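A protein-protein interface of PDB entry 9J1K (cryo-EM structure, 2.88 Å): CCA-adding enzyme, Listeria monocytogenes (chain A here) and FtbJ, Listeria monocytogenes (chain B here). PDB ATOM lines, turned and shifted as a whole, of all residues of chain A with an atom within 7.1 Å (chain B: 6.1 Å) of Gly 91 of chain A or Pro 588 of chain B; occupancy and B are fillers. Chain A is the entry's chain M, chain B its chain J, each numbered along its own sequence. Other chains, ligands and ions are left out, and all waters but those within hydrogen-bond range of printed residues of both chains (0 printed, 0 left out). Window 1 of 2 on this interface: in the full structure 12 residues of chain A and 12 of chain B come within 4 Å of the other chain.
Among the printed residues, pairs that only touch across the chains: Thr 86 of chain A with Pro 588 of chain B, Gly 91 of chain A with Val 589 of chain B, Gly 91 of chain A with Ile 590 of chain B, Leu 93 of chain A with Val 589 of chain B and Leu 93 of chain A with Ile 590 of chain B.
Hydrophobic or aromatic side chains of chain A that line the printed part of chain B: Leu 93. Among the printed residues, 8 pairs touch across the chains.
The backbone carbonyl oxygen (O) of Thr 86 of chain A sits close to the side-chain amide oxygen (OD1) of Asn 89 of chain A. N of Glu 99 of chain A lies within hydrogen-bond range of O of Glu 92 of chain A.
The backbone NH of Gly 91 of chain A lies within hydrogen-bond range of the backbone carbonyl oxygen of Pro 588 of chain B, at 3.0 Å. The backbone NH of Glu 92 of chain A is in hydrogen-bond range of the backbone carbonyl oxygen of Ile 590 of chain B, at 3.2 Å. The backbone carbonyl oxygen (O) of Ala 90 of chain A sits close to the backbone carbonyl oxygen (O) of Pro 588 of chain B (3.4 Å).
Printed residues of chain B within 4 Å of Ala 90 of chain A: Pro 588. Of the printed residues of chain B, Gly 91 of chain A touches Pro 588, Val 589 and Ile 590. Of the printed residues of chain B, Glu 92 of chain A touches Ile 590 (3.2 Å). Printed residues of chain B within 4 Å of Leu 93 of chain A: Val 589 (3.9 Å) and Ile 590 (3.6 Å). Lys 97 of chain A touches none of the printed residues of chain B. Gln 585 of chain B touches none of the printed residues of chain A. Pro 588 of chain B touches just these residues of chain A: Thr 86 (3.9 Å), Ala 90 (3.0 Å) and Gly 91 (3.0 Å). The nearest printed residue of chain B that does not touch Gly 91 of chain A is Asn 587 of chain B (7.3 Å). The nearest residue of chain A that does not touch Pro 588 of chain B is Asn 89 of chain A (4.9 Å).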
ATOM      1  N   THR A  86      22.335 -16.578  -4.250  1.00  0.00           N
ATOM      2  CA  THR A  86      21.582 -17.827  -4.335  1.00  0.00           C
ATOM      3  C   THR A  86      20.081 -17.563  -4.323  1.00  0.00           C
ATOM      4  O   THR A  86      19.321 -18.234  -5.033  1.00  0.00           O
ATOM      5  CB  THR A  86      21.986 -18.756  -3.187  1.00  0.00           C
ATOM      6  OG1 THR A  86      23.271 -19.328  -3.465  1.00  0.00           O
ATOM      7  CG2 THR A  86      20.974 -19.880  -3.009  1.00  0.00           C
ATOM      8  N   VAL A  87      19.638 -16.576  -3.538  1.00  0.00           N
ATOM      9  CA  VAL A  87      18.219 -16.231  -3.483  1.00  0.00           C
ATOM     10  C   VAL A  87      17.704 -15.796  -4.852  1.00  0.00           C
ATOM     11  O   VAL A  87      16.530 -16.013  -5.181  1.00  0.00           O
ATOM     12  CB  VAL A  87      17.994 -15.147  -2.406  1.00  0.00           C
ATOM     13  CG1 VAL A  87      16.788 -14.273  -2.730  1.00  0.00           C
ATOM     14  CG2 VAL A  87      17.838 -15.789  -1.035  1.00  0.00           C
ATOM     15  N   THR A  88      18.573 -15.199  -5.675  1.00  0.00           N
ATOM     16  CA  THR A  88      18.163 -14.694  -6.986  1.00  0.00           C
ATOM     17  C   THR A  88      17.416 -15.744  -7.809  1.00  0.00           C
ATOM     18  O   THR A  88      16.376 -15.454  -8.411  1.00  0.00           O
ATOM     19  CB  THR A  88      19.382 -14.210  -7.777  1.00  0.00           C
ATOM     20  OG1 THR A  88      20.324 -15.282  -7.913  1.00  0.00           O
ATOM     21  CG2 THR A  88      20.049 -13.036  -7.101  1.00  0.00           C
ATOM     22  N   ASN A  89      17.942 -16.971  -7.847  1.00  0.00           N
ATOM     23  CA  ASN A  89      17.530 -17.935  -8.868  1.00  0.00           C
ATOM     24  C   ASN A  89      16.053 -18.303  -8.753  1.00  0.00           C
ATOM     25  O   ASN A  89      15.337 -18.338  -9.761  1.00  0.00           O
ATOM     26  CB  ASN A  89      18.404 -19.186  -8.782  1.00  0.00           C
ATOM     27  CG  ASN A  89      19.882 -18.859  -8.749  1.00  0.00           C
ATOM     28  OD1 ASN A  89      20.416 -18.436  -7.724  1.00  0.00           O
ATOM     29  ND2 ASN A  89      20.554 -19.051  -9.878  1.00  0.00           N
ATOM     30  N   ALA A  90      15.587 -18.600  -7.537  1.00  0.00           N
ATOM     31  CA  ALA A  90      14.208 -19.012  -7.274  1.00  0.00           C
ATOM     32  C   ALA A  90      13.853 -20.336  -7.949  1.00  0.00           C
ATOM     33  O   ALA A  90      14.607 -20.846  -8.784  1.00  0.00           O
ATOM     34  CB  ALA A  90      13.221 -17.919  -7.700  1.00  0.00           C
ATOM     35  N   GLY A  91      12.706 -20.903  -7.576  1.00  0.00           N
ATOM     36  CA  GLY A  91      12.313 -22.238  -7.992  1.00  0.00           C
ATOM     37  C   GLY A  91      11.132 -22.316  -8.940  1.00  0.00           C
ATOM     38  O   GLY A  91      11.290 -22.212 -10.160  1.00  0.00           O
ATOM     39  N   GLU A  92       9.944 -22.524  -8.370  1.00  0.00           N
ATOM     40  CA  GLU A  92       8.683 -22.732  -9.089  1.00  0.00           C
ATOM     41  C   GLU A  92       8.840 -23.756 -10.225  1.00  0.00           C
ATOM     42  O   GLU A  92       8.710 -23.472 -11.415  1.00  0.00           O
ATOM     43  CB  GLU A  92       8.051 -21.401  -9.542  1.00  0.00           C
ATOM     44  CG  GLU A  92       8.583 -20.660 -10.781  1.00  0.00           C
ATOM     45  CD  GLU A  92       9.563 -19.541 -10.464  1.00  0.00           C
ATOM     46  OE1 GLU A  92      10.442 -19.703  -9.597  1.00  0.00           O
ATOM     47  OE2 GLU A  92       9.446 -18.473 -11.098  1.00  0.00           O
ATOM     48  N   LEU A  93       9.117 -24.988  -9.800  1.00  0.00           N
ATOM     49  CA  LEU A  93       9.065 -26.137 -10.693  1.00  0.00           C
ATOM     50  C   LEU A  93       7.617 -26.551 -10.928  1.00  0.00           C
ATOM     51  O   LEU A  93       6.798 -26.538 -10.005  1.00  0.00           O
ATOM     52  CB  LEU A  93       9.844 -27.312 -10.101  1.00  0.00           C
ATOM     53  CG  LEU A  93      11.371 -27.326 -10.198  1.00  0.00           C
ATOM     54  CD1 LEU A  93      11.902 -28.747 -10.064  1.00  0.00           C
ATOM     55  CD2 LEU A  93      11.845 -26.698 -11.490  1.00  0.00           C
ATOM     56  N   LYS A  94       7.298 -26.926 -12.169  1.00  0.00           N
ATOM     57  CA  LYS A  94       5.941 -27.384 -12.472  1.00  0.00           C
ATOM     58  C   LYS A  94       5.740 -28.817 -11.990  1.00  0.00           C
ATOM     59  O   LYS A  94       4.965 -29.075 -11.064  1.00  0.00           O
ATOM     60  CB  LYS A  94       5.680 -27.283 -13.981  1.00  0.00           C
ATOM     61  CG  LYS A  94       4.890 -26.063 -14.465  1.00  0.00           C
ATOM     62  CD  LYS A  94       3.818 -25.558 -13.504  1.00  0.00           C
ATOM     63  CE  LYS A  94       2.720 -26.585 -13.243  1.00  0.00           C
ATOM     64  NZ  LYS A  94       1.655 -26.039 -12.360  1.00  0.00           N
ATOM     65  N   LYS A  97      10.168 -29.483 -14.893  1.00  0.00           N
ATOM     66  CA  LYS A  97      10.660 -28.372 -15.695  1.00  0.00           C
ATOM     67  C   LYS A  97      10.643 -27.077 -14.889  1.00  0.00           C
ATOM     68  O   LYS A  97       9.867 -26.914 -13.944  1.00  0.00           O
ATOM     69  CB  LYS A  97       9.840 -28.173 -16.983  1.00  0.00           C
ATOM     70  CG  LYS A  97       9.578 -29.378 -17.926  1.00  0.00           C
ATOM     71  CD  LYS A  97       8.930 -30.617 -17.318  1.00  0.00           C
ATOM     72  CE  LYS A  97       7.616 -30.275 -16.632  1.00  0.00           C
ATOM     73  NZ  LYS A  97       7.011 -31.465 -15.976  1.00  0.00           N
ATOM     74  N   VAL A  98      11.506 -26.147 -15.287  1.00  0.00           N
ATOM     75  CA  VAL A  98      11.635 -24.865 -14.603  1.00  0.00           C
ATOM     76  C   VAL A  98      10.553 -23.923 -15.118  1.00  0.00           C
ATOM     77  O   VAL A  98      10.382 -23.764 -16.331  1.00  0.00           O
ATOM     78  CB  VAL A  98      13.036 -24.270 -14.805  1.00  0.00           C
ATOM     79  CG1 VAL A  98      12.998 -22.752 -14.709  1.00  0.00           C
ATOM     80  CG2 VAL A  98      14.006 -24.848 -13.790  1.00  0.00           C
ATOM     81  N   GLU A  99       9.820 -23.306 -14.194  1.00  0.00           N
ATOM     82  CA  GLU A  99       8.756 -22.359 -14.521  1.00  0.00           C
ATOM     83  C   GLU A  99       7.726 -22.964 -15.468  1.00  0.00           C
ATOM     84  O   GLU A  99       6.732 -23.539 -15.027  1.00  0.00           O
ATOM     85  CB  GLU A  99       9.342 -21.080 -15.127  1.00  0.00           C
ATOM     86  CG  GLU A  99      10.122 -20.229 -14.136  1.00  0.00           C
ATOM     87  CD  GLU A  99      11.409 -19.683 -14.718  1.00  0.00           C
ATOM     88  OE1 GLU A  99      11.590 -19.765 -15.950  1.00  0.00           O
ATOM     89  OE2 GLU A  99      12.238 -19.165 -13.941  1.00  0.00           O
ATOM     90  N   GLN B 585      22.478 -23.280   2.785  1.00  0.00           N
ATOM     91  CA  GLN B 585      22.450 -24.580   2.117  1.00  0.00           C
ATOM     92  C   GLN B 585      21.120 -24.805   1.394  1.00  0.00           C
ATOM     93  O   GLN B 585      21.112 -25.277   0.252  1.00  0.00           O
ATOM     94  CB  GLN B 585      22.721 -25.668   3.168  1.00  0.00           C
ATOM     95  CG  GLN B 585      22.354 -27.145   2.902  1.00  0.00           C
ATOM     96  CD  GLN B 585      22.414 -27.583   1.450  1.00  0.00           C
ATOM     97  OE1 GLN B 585      21.386 -27.795   0.806  1.00  0.00           O
ATOM     98  NE2 GLN B 585      23.626 -27.730   0.930  1.00  0.00           N
ATOM     99  N   LYS B 586      20.006 -24.395   2.009  1.00  0.00           N
ATOM    100  CA  LYS B 586      18.666 -24.729   1.528  1.00  0.00           C
ATOM    101  C   LYS B 586      18.496 -24.471   0.033  1.00  0.00           C
ATOM    102  O   LYS B 586      18.884 -23.422  -0.491  1.00  0.00           O
ATOM    103  CB  LYS B 586      17.621 -23.932   2.315  1.00  0.00           C
ATOM    104  CG  LYS B 586      17.824 -22.424   2.257  1.00  0.00           C
ATOM    105  CD  LYS B 586      16.745 -21.669   3.018  1.00  0.00           C
ATOM    106  CE  LYS B 586      16.836 -21.889   4.515  1.00  0.00           C
ATOM    107  NZ  LYS B 586      16.117 -20.819   5.261  1.00  0.00           N
ATOM    108  N   ASN B 587      17.910 -25.455  -0.646  1.00  0.00           N
ATOM    109  CA  ASN B 587      17.660 -25.360  -2.080  1.00  0.00           C
ATOM    110  C   ASN B 587      16.653 -24.255  -2.372  1.00  0.00           C
ATOM    111  O   ASN B 587      15.567 -24.241  -1.782  1.00  0.00           O
ATOM    112  CB  ASN B 587      17.131 -26.694  -2.608  1.00  0.00           C
ATOM    113  CG  ASN B 587      17.588 -26.990  -4.022  1.00  0.00           C
ATOM    114  OD1 ASN B 587      18.676 -26.592  -4.434  1.00  0.00           O
ATOM    115  ND2 ASN B 587      16.748 -27.690  -4.777  1.00  0.00           N
ATOM    116  N   PRO B 588      16.959 -23.332  -3.279  1.00  0.00           N
ATOM    117  CA  PRO B 588      16.014 -22.272  -3.653  1.00  0.00           C
ATOM    118  C   PRO B 588      14.993 -22.734  -4.689  1.00  0.00           C
ATOM    119  O   PRO B 588      14.679 -22.019  -5.640  1.00  0.00           O
ATOM    120  CB  PRO B 588      16.935 -21.181  -4.204  1.00  0.00           C
ATOM    121  CG  PRO B 588      18.099 -21.935  -4.781  1.00  0.00           C
ATOM    122  CD  PRO B 588      18.202 -23.265  -4.066  1.00  0.00           C
ATOM    123  N   VAL B 589      14.467 -23.940  -4.498  1.00  0.00           N
ATOM    124  CA  VAL B 589      13.489 -24.539  -5.395  1.00  0.00           C
ATOM    125  C   VAL B 589      12.213 -24.758  -4.598  1.00  0.00           C
ATOM    126  O   VAL B 589      12.229 -25.440  -3.565  1.00  0.00           O
ATOM    127  CB  VAL B 589      13.993 -25.860  -5.996  1.00  0.00           C
ATOM    128  CG1 VAL B 589      12.856 -26.603  -6.680  1.00  0.00           C
ATOM    129  CG2 VAL B 589      15.132 -25.600  -6.970  1.00  0.00           C
ATOM    130  N   ILE B 590      11.113 -24.179  -5.070  1.00  0.00           N
ATOM    131  CA  ILE B 590       9.823 -24.275  -4.400  1.00  0.00           C
ATOM    132  C   ILE B 590       8.886 -25.053  -5.319  1.00  0.00           C
ATOM    133  O   ILE B 590       8.421 -24.536  -6.342  1.00  0.00           O
ATOM    134  CB  ILE B 590       9.264 -22.890  -4.037  1.00  0.00           C
ATOM    135  CG1 ILE B 590       7.777 -22.972  -3.685  1.00  0.00           C
ATOM    136  CG2 ILE B 590       9.537 -21.879  -5.147  1.00  0.00           C
ATOM    137  CD1 ILE B 590       7.476 -23.828  -2.472  1.00  0.00           C
